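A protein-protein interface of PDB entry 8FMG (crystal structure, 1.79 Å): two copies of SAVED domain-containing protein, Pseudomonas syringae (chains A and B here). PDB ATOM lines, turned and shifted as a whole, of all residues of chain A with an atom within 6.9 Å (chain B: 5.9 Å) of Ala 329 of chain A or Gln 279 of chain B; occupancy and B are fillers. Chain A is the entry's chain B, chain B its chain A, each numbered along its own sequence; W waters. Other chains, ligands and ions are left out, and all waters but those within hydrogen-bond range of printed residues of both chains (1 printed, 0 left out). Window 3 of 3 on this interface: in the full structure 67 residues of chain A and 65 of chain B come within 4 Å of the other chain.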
ATOM      1  N   GLN A 321     -18.738  37.542  -6.662  1.00  0.00           N
ATOM      2  CA  GLN A 321     -18.647  36.317  -5.876  1.00  0.00           C
ATOM      3  C   GLN A 321     -19.711  35.307  -6.302  1.00  0.00           C
ATOM      4  O   GLN A 321     -19.443  34.100  -6.343  1.00  0.00           O
ATOM      5  CB  GLN A 321     -18.741  36.634  -4.388  1.00  0.00           C
ATOM      6  CG  GLN A 321     -18.539  35.413  -3.523  1.00  0.00           C
ATOM      7  CD  GLN A 321     -19.837  34.688  -3.277  1.00  0.00           C
ATOM      8  OE1 GLN A 321     -20.884  35.318  -3.139  1.00  0.00           O
ATOM      9  NE2 GLN A 321     -19.787  33.362  -3.238  1.00  0.00           N
ATOM     10  N   ARG A 323     -20.722  34.798  -9.288  1.00  0.00           N
ATOM     11  CA  ARG A 323     -20.276  34.178 -10.530  1.00  0.00           C
ATOM     12  C   ARG A 323     -19.020  33.335 -10.347  1.00  0.00           C
ATOM     13  O   ARG A 323     -18.845  32.337 -11.052  1.00  0.00           O
ATOM     14  CB  ARG A 323     -20.001  35.252 -11.589  1.00  0.00           C
ATOM     15  CG  ARG A 323     -21.186  36.131 -11.926  1.00  0.00           C
ATOM     16  CD  ARG A 323     -22.366  35.315 -12.429  1.00  0.00           C
ATOM     17  NE  ARG A 323     -23.479  36.161 -12.833  1.00  0.00           N
ATOM     18  CZ  ARG A 323     -24.654  35.705 -13.252  1.00  0.00           C
ATOM     19  NH1 ARG A 323     -24.906  34.410 -13.322  1.00  0.00           N
ATOM     20  NH2 ARG A 323     -25.598  36.573 -13.608  1.00  0.00           N
ATOM     21  N   LEU A 324     -18.123  33.743  -9.447  1.00  0.00           N
ATOM     22  CA  LEU A 324     -16.947  32.928  -9.162  1.00  0.00           C
ATOM     23  C   LEU A 324     -17.355  31.584  -8.571  1.00  0.00           C
ATOM     24  O   LEU A 324     -16.795  30.542  -8.930  1.00  0.00           O
ATOM     25  CB  LEU A 324     -16.002  33.674  -8.216  1.00  0.00           C
ATOM     26  CG  LEU A 324     -15.381  34.964  -8.752  1.00  0.00           C
ATOM     27  CD1 LEU A 324     -14.237  35.447  -7.859  1.00  0.00           C
ATOM     28  CD2 LEU A 324     -14.885  34.804 -10.185  1.00  0.00           C
ATOM     29  N   SER A 325     -18.347  31.590  -7.671  1.00  0.00           N
ATOM     30  CA  SER A 325     -18.893  30.339  -7.159  1.00  0.00           C
ATOM     31  C   SER A 325     -19.431  29.473  -8.290  1.00  0.00           C
ATOM     32  O   SER A 325     -19.267  28.248  -8.282  1.00  0.00           O
ATOM     33  CB  SER A 325     -19.997  30.636  -6.146  1.00  0.00           C
ATOM     34  OG  SER A 325     -20.664  29.451  -5.757  1.00  0.00           O
ATOM     35  N   GLN A 326     -20.091  30.096  -9.267  1.00  0.00           N
ATOM     36  CA  GLN A 326     -20.593  29.345 -10.411  1.00  0.00           C
ATOM     37  C   GLN A 326     -19.453  28.764 -11.237  1.00  0.00           C
ATOM     38  O   GLN A 326     -19.519  27.602 -11.657  1.00  0.00           O
ATOM     39  CB  GLN A 326     -21.471  30.245 -11.274  1.00  0.00           C
ATOM     40  CG  GLN A 326     -22.789  30.636 -10.637  1.00  0.00           C
ATOM     41  CD  GLN A 326     -23.591  31.558 -11.528  1.00  0.00           C
ATOM     42  OE1 GLN A 326     -23.179  31.871 -12.644  1.00  0.00           O
ATOM     43  NE2 GLN A 326     -24.743  32.001 -11.039  1.00  0.00           N
ATOM     44  N   LEU A 327     -18.399  29.549 -11.475  1.00  0.00           N
ATOM     45  CA  LEU A 327     -17.314  29.095 -12.340  1.00  0.00           C
ATOM     46  C   LEU A 327     -16.473  28.018 -11.664  1.00  0.00           C
ATOM     47  O   LEU A 327     -16.044  27.058 -12.313  1.00  0.00           O
ATOM     48  CB  LEU A 327     -16.429  30.277 -12.740  1.00  0.00           C
ATOM     49  CG  LEU A 327     -17.114  31.336 -13.602  1.00  0.00           C
ATOM     50  CD1 LEU A 327     -16.214  32.550 -13.749  1.00  0.00           C
ATOM     51  CD2 LEU A 327     -17.484  30.796 -14.972  1.00  0.00           C
ATOM     52  N   GLU A 328     -16.217  28.170 -10.361  1.00  0.00           N
ATOM     53  CA  GLU A 328     -15.470  27.152  -9.632  1.00  0.00           C
ATOM     54  C   GLU A 328     -16.244  25.844  -9.554  1.00  0.00           C
ATOM     55  O   GLU A 328     -15.639  24.766  -9.527  1.00  0.00           O
ATOM     56  CB  GLU A 328     -15.127  27.668  -8.232  1.00  0.00           C
ATOM     57  CG  GLU A 328     -14.267  28.926  -8.259  1.00  0.00           C
ATOM     58  CD  GLU A 328     -13.850  29.410  -6.879  1.00  0.00           C
ATOM     59  OE1 GLU A 328     -14.149  28.715  -5.885  1.00  0.00           O
ATOM     60  OE2 GLU A 328     -13.223  30.486  -6.802  1.00  0.00           O
ATOM     61  N   ALA A 329     -17.578  25.913  -9.522  1.00  0.00           N
ATOM     62  CA  ALA A 329     -18.364  24.692  -9.618  1.00  0.00           C
ATOM     63  C   ALA A 329     -18.192  24.043 -10.984  1.00  0.00           C
ATOM     64  O   ALA A 329     -18.229  22.811 -11.096  1.00  0.00           O
ATOM     65  CB  ALA A 329     -19.838  24.986  -9.348  1.00  0.00           C
ATOM     66  N   LEU A 330     -17.977  24.845 -12.028  1.00  0.00           N
ATOM     67  CA  LEU A 330     -17.862  24.279 -13.361  1.00  0.00           C
ATOM     68  C   LEU A 330     -16.567  23.497 -13.550  1.00  0.00           C
ATOM     69  O   LEU A 330     -16.522  22.578 -14.377  1.00  0.00           O
ATOM     70  CB  LEU A 330     -17.949  25.382 -14.410  1.00  0.00           C
ATOM     71  CG  LEU A 330     -19.338  25.971 -14.654  1.00  0.00           C
ATOM     72  CD1 LEU A 330     -19.212  27.159 -15.589  1.00  0.00           C
ATOM     73  CD2 LEU A 330     -20.265  24.915 -15.220  1.00  0.00           C
ATOM     74  N   THR A 331     -15.505  23.835 -12.816  1.00  0.00           N
ATOM     75  CA  THR A 331     -14.210  23.233 -13.098  1.00  0.00           C
ATOM     76  C   THR A 331     -13.312  23.337 -11.879  1.00  0.00           C
ATOM     77  O   THR A 331     -13.366  24.338 -11.158  1.00  0.00           O
ATOM     78  CB  THR A 331     -13.527  23.916 -14.290  1.00  0.00           C
ATOM     79  OG1 THR A 331     -12.177  23.453 -14.403  1.00  0.00           O
ATOM     80  CG2 THR A 331     -13.504  25.425 -14.099  1.00  0.00           C
ATOM     81  N   PRO A 332     -12.451  22.341 -11.645  1.00  0.00           N
ATOM     82  CA  PRO A 332     -11.415  22.491 -10.611  1.00  0.00           C
ATOM     83  C   PRO A 332     -10.200  23.278 -11.074  1.00  0.00           C
ATOM     84  O   PRO A 332      -9.334  23.587 -10.246  1.00  0.00           O
ATOM     85  CB  PRO A 332     -11.026  21.035 -10.305  1.00  0.00           C
ATOM     86  CG  PRO A 332     -11.186  20.353 -11.635  1.00  0.00           C
ATOM     87  CD  PRO A 332     -12.384  21.016 -12.298  1.00  0.00           C
ATOM     88  N   HIS A 359      -9.256  29.073  -4.364  1.00  0.00           N
ATOM     89  CA  HIS A 359      -9.202  28.516  -5.705  1.00  0.00           C
ATOM     90  C   HIS A 359      -8.103  29.268  -6.437  1.00  0.00           C
ATOM     91  O   HIS A 359      -7.817  30.428  -6.125  1.00  0.00           O
ATOM     92  CB  HIS A 359     -10.551  28.679  -6.410  1.00  0.00           C
ATOM     93  CG  HIS A 359     -10.675  27.932  -7.701  1.00  0.00           C
ATOM     94  ND1 HIS A 359     -11.404  26.766  -7.817  1.00  0.00           N
ATOM     95  CD2 HIS A 359     -10.215  28.212  -8.944  1.00  0.00           C
ATOM     96  CE1 HIS A 359     -11.367  26.349  -9.069  1.00  0.00           C
ATOM     97  NE2 HIS A 359     -10.652  27.209  -9.773  1.00  0.00           N
ATOM     98  N   VAL B 273     -24.110  18.451   2.662  1.00  0.00           N
ATOM     99  CA  VAL B 273     -23.457  19.579   2.011  1.00  0.00           C
ATOM    100  C   VAL B 273     -24.374  20.788   2.106  1.00  0.00           C
ATOM    101  O   VAL B 273     -25.551  20.718   1.729  1.00  0.00           O
ATOM    102  CB  VAL B 273     -23.123  19.263   0.540  1.00  0.00           C
ATOM    103  CG1 VAL B 273     -22.485  20.470  -0.125  1.00  0.00           C
ATOM    104  CG2 VAL B 273     -22.219  18.052   0.461  1.00  0.00           C
ATOM    105  N   SER B 275     -24.718  24.480   0.706  1.00  0.00           N
ATOM    106  CA  SER B 275     -24.290  25.435  -0.313  1.00  0.00           C
ATOM    107  C   SER B 275     -25.159  26.681  -0.176  1.00  0.00           C
ATOM    108  O   SER B 275     -26.150  26.861  -0.884  1.00  0.00           O
ATOM    109  CB  SER B 275     -24.384  24.814  -1.677  1.00  0.00           C
ATOM    110  OG  SER B 275     -23.447  23.765  -1.793  1.00  0.00           O
ATOM    111  N   ILE B 276     -24.778  27.538   0.769  1.00  0.00           N
ATOM    112  CA  ILE B 276     -25.493  28.776   1.063  1.00  0.00           C
ATOM    113  C   ILE B 276     -24.659  29.986   0.664  1.00  0.00           C
ATOM    114  O   ILE B 276     -25.114  30.848  -0.088  1.00  0.00           O
ATOM    115  CB  ILE B 276     -25.881  28.842   2.558  1.00  0.00           C
ATOM    116  CG1 ILE B 276     -26.551  27.551   3.025  1.00  0.00           C
ATOM    117  CG2 ILE B 276     -26.780  30.045   2.805  1.00  0.00           C
ATOM    118  CD1 ILE B 276     -27.888  27.265   2.390  1.00  0.00           C
ATOM    119  N   SER B 277     -23.435  30.080   1.194  1.00  0.00           N
ATOM    120  CA  SER B 277     -22.516  31.137   0.801  1.00  0.00           C
ATOM    121  C   SER B 277     -22.001  30.929  -0.611  1.00  0.00           C
ATOM    122  O   SER B 277     -21.639  31.890  -1.295  1.00  0.00           O
ATOM    123  CB  SER B 277     -21.321  31.176   1.750  1.00  0.00           C
ATOM    124  OG  SER B 277     -21.724  31.397   3.086  1.00  0.00           O
ATOM    125  N   ALA B 278     -21.932  29.679  -1.042  1.00  0.00           N
ATOM    126  CA  ALA B 278     -21.346  29.338  -2.324  1.00  0.00           C
ATOM    127  C   ALA B 278     -21.765  27.912  -2.636  1.00  0.00           C
ATOM    128  O   ALA B 278     -22.298  27.201  -1.780  1.00  0.00           O
ATOM    129  CB  ALA B 278     -19.823  29.490  -2.297  1.00  0.00           C
ATOM    130  N   GLN B 279     -21.530  27.508  -3.877  1.00  0.00           N
ATOM    131  CA  GLN B 279     -21.788  26.133  -4.285  1.00  0.00           C
ATOM    132  C   GLN B 279     -20.587  25.274  -3.901  1.00  0.00           C
ATOM    133  O   GLN B 279     -19.471  25.505  -4.381  1.00  0.00           O
ATOM    134  CB  GLN B 279     -22.045  26.048  -5.786  1.00  0.00           C
ATOM    135  CG  GLN B 279     -22.286  24.629  -6.300  1.00  0.00           C
ATOM    136  CD  GLN B 279     -23.517  23.983  -5.689  1.00  0.00           C
ATOM    137  OE1 GLN B 279     -24.594  24.581  -5.664  1.00  0.00           O
ATOM    138  NE2 GLN B 279     -23.363  22.764  -5.187  1.00  0.00           N
ATOM    139  N   VAL B 280     -20.814  24.296  -3.030  1.00  0.00           N
ATOM    140  CA  VAL B 280     -19.769  23.356  -2.630  1.00  0.00           C
ATOM    141  C   VAL B 280     -19.653  22.306  -3.729  1.00  0.00           C
ATOM    142  O   VAL B 280     -20.602  21.538  -3.943  1.00  0.00           O
ATOM    143  CB  VAL B 280     -20.088  22.713  -1.272  1.00  0.00           C
ATOM    144  CG1 VAL B 280     -19.100  21.607  -0.967  1.00  0.00           C
ATOM    145  CG2 VAL B 280     -20.054  23.752  -0.171  1.00  0.00           C
ATOM    146  N   PRO B 281     -18.535  22.231  -4.453  1.00  0.00           N
ATOM    147  CA  PRO B 281     -18.428  21.224  -5.525  1.00  0.00           C
ATOM    148  C   PRO B 281     -18.421  19.818  -4.940  1.00  0.00           C
ATOM    149  O   PRO B 281     -17.584  19.493  -4.093  1.00  0.00           O
ATOM    150  CB  PRO B 281     -17.097  21.567  -6.212  1.00  0.00           C
ATOM    151  CG  PRO B 281     -16.747  22.970  -5.745  1.00  0.00           C
ATOM    152  CD  PRO B 281     -17.329  23.079  -4.365  1.00  0.00           C
ATOM    153  N   VAL B 282     -19.360  18.977  -5.394  1.00  0.00           N
ATOM    154  CA  VAL B 282     -19.474  17.635  -4.835  1.00  0.00           C
ATOM    155  C   VAL B 282     -18.225  16.806  -5.098  1.00  0.00           C
ATOM    156  O   VAL B 282     -17.948  15.851  -4.361  1.00  0.00           O
ATOM    157  CB  VAL B 282     -20.727  16.920  -5.384  1.00  0.00           C
ATOM    158  CG1 VAL B 282     -21.984  17.654  -4.943  1.00  0.00           C
ATOM    159  CG2 VAL B 282     -20.677  16.812  -6.899  1.00  0.00           C
ATOM    160  N   ARG B 283     -17.452  17.147  -6.134  1.00  0.00           N
ATOM    161  CA  ARG B 283     -16.188  16.457  -6.355  1.00  0.00           C
ATOM    162  C   ARG B 283     -15.260  16.593  -5.151  1.00  0.00           C
ATOM    163  O   ARG B 283     -14.490  15.672  -4.852  1.00  0.00           O
ATOM    164  CB  ARG B 283     -15.513  16.996  -7.615  1.00  0.00           C
ATOM    165  CG  ARG B 283     -15.001  18.425  -7.486  1.00  0.00           C
ATOM    166  CD  ARG B 283     -14.634  19.051  -8.841  1.00  0.00           C
ATOM    167  NE  ARG B 283     -14.034  20.365  -8.646  1.00  0.00           N
ATOM    168  CZ  ARG B 283     -14.603  21.523  -8.965  1.00  0.00           C
ATOM    169  NH1 ARG B 283     -15.714  21.578  -9.686  1.00  0.00           N
ATOM    170  NH2 ARG B 283     -14.047  22.656  -8.543  1.00  0.00           N
ATOM    171  N   GLU B 296     -27.884  17.578   0.131  1.00  0.00           N
ATOM    172  CA  GLU B 296     -27.475  18.960  -0.065  1.00  0.00           C
ATOM    173  C   GLU B 296     -28.623  19.898   0.255  1.00  0.00           C
ATOM    174  O   GLU B 296     -29.749  19.696  -0.213  1.00  0.00           O
ATOM    175  CB  GLU B 296     -26.987  19.180  -1.501  1.00  0.00           C
ATOM    176  CG  GLU B 296     -26.481  20.585  -1.759  1.00  0.00           C
ATOM    177  CD  GLU B 296     -25.660  20.693  -3.029  1.00  0.00           C
ATOM    178  OE1 GLU B 296     -25.826  19.847  -3.930  1.00  0.00           O
ATOM    179  OE2 GLU B 296     -24.840  21.631  -3.116  1.00  0.00           O
ATOM    180  N   SER B 298     -29.321  23.944  -0.130  1.00  0.00           N
ATOM    181  CA  SER B 298     -28.770  25.060  -0.880  1.00  0.00           C
ATOM    182  C   SER B 298     -29.832  26.132  -1.047  1.00  0.00           C
ATOM    183  O   SER B 298     -31.002  25.937  -0.720  1.00  0.00           O
ATOM    184  CB  SER B 298     -28.260  24.587  -2.248  1.00  0.00           C
ATOM    185  OG  SER B 298     -29.328  24.038  -3.002  1.00  0.00           O
ATOM    186  N   PRO B 302     -26.386  30.978  -4.372  1.00  0.00           N
ATOM    187  CA  PRO B 302     -25.452  31.055  -3.241  1.00  0.00           C
ATOM    188  C   PRO B 302     -24.618  32.324  -3.295  1.00  0.00           C
ATOM    189  O   PRO B 302     -24.096  32.706  -4.345  1.00  0.00           O
ATOM    190  CB  PRO B 302     -24.584  29.797  -3.407  1.00  0.00           C
ATOM    191  CG  PRO B 302     -25.455  28.853  -4.177  1.00  0.00           C
ATOM    192  CD  PRO B 302     -26.237  29.719  -5.126  1.00  0.00           C
ATOM    193  N   ALA B 340     -20.400  25.560   3.196  1.00  0.00           N
ATOM    194  CA  ALA B 340     -20.034  26.904   2.777  1.00  0.00           C
ATOM    195  C   ALA B 340     -21.210  27.775   3.207  1.00  0.00           C
ATOM    196  O   ALA B 340     -22.176  27.947   2.466  1.00  0.00           O
ATOM    197  CB  ALA B 340     -19.777  26.990   1.285  1.00  0.00           C
ATOM    198  N   ARG B 366     -12.179  23.428   4.780  1.00  0.00           N
ATOM    199  CA  ARG B 366     -11.111  23.614   3.807  1.00  0.00           C
ATOM    200  C   ARG B 366      -9.757  23.712   4.505  1.00  0.00           C
ATOM    201  O   ARG B 366      -9.622  24.373   5.543  1.00  0.00           O
ATOM    202  CB  ARG B 366     -11.365  24.875   2.981  1.00  0.00           C
ATOM    203  CG  ARG B 366     -12.631  24.825   2.151  1.00  0.00           C
ATOM    204  CD  ARG B 366     -12.479  23.840   1.018  1.00  0.00           C
ATOM    205  NE  ARG B 366     -13.624  23.854   0.115  1.00  0.00           N
ATOM    206  CZ  ARG B 366     -13.677  23.188  -1.028  1.00  0.00           C
ATOM    207  NH1 ARG B 366     -12.639  22.508  -1.476  1.00  0.00           N
ATOM    208  NH2 ARG B 366     -14.806  23.197  -1.730  1.00  0.00           N
HETATM  209  O   HOH W   1     -18.214  26.694  -6.182  1.00  0.00           O
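Hydrophobic or aromatic side chains of chain B that line the printed part of chain A: Ala 278.
Hydrophobic or aromatic side chains of chain A that line the printed part of chain B: Ala 329 and Pro 332.
No position is printed for both chains.
The guanidinium group (NH2) of Arg 283 of chain B is in hydrogen-bond range of the backbone carbonyl oxygen (O) of Glu 328 of chain A.
O of Ser 277 of chain B is in hydrogen-bond range of NE2 of Gln 321 of chain A (3.1 Å).
The guanidinium group (NH1) of Arg 283 of chain B lies within hydrogen-bond range of the backbone carbonyl oxygen (O) of Ala 329 of chain A (3.1 Å).
The backbone carbonyl oxygen of Thr 331 of chain A lies within hydrogen-bond range of the guanidinium group of Arg 283 of chain B (3.2 Å).
The backbone NH of Gln 279 of chain B sits at hydrogen-bond distance from the side-chain hydroxyl of Ser 325 of chain A, at 2.8 Å.
Printed residues of chain B within 4 Å of Gln 321 of chain A: Ser 277 and Ala 278.
Leu 327 of chain A touches none of the printed residues of chain B.
Printed residues of chain B within 4 Å of Pro 332 of chain A: Arg 283 (3.4 Å).
Ile 276 of chain B touches none of the printed residues of chain A.
Of the printed residues of chain A, Ser 277 of chain B touches Gln 321.
Of the printed residues of chain A, Ala 278 of chain B touches Gln 321 and Ser 325.
Of the printed residues of chain A, Gln 279 of chain B touches Ser 325 and Ala 329.
Printed residues of chain A within 4 Å of Arg 283 of chain B: Glu 328, Ala 329, Thr 331 and Pro 332.
The nearest residue of chain B that does not touch Ala 329 of chain A is Pro 281 of chain B (4.5 Å).
The nearest printed residue of chain A that does not touch Ser 277 of chain B is Ser 325 of chain A (5.2 Å).
The backbone NH of Ser 277 of chain B is in hydrogen-bond range of the backbone carbonyl oxygen of Ala 340 of chain B (2.8 Å).
NE2 of Gln 279 of chain B lies within hydrogen-bond range of OE2 of Glu 296 of chain B.
Water W1 lies within hydrogen-bond range of O of Gln 279 of chain B, O of Ser 325 of chain A and N of Ala 329 of chain A.
CB of Ala 278 of chain B touches NE2 of Gln 321 of chain A (3.98 Å).
Ala 278 of chain B touches Ser 325 of chain A (CA to OG, 3.5 Å).
Gln 279 of chain B touches Ala 329 of chain A (CG to CB, 3.9 Å).
CA of Pro 332 of chain A touches NH2 of Arg 283 of chain B (3.4 Å).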
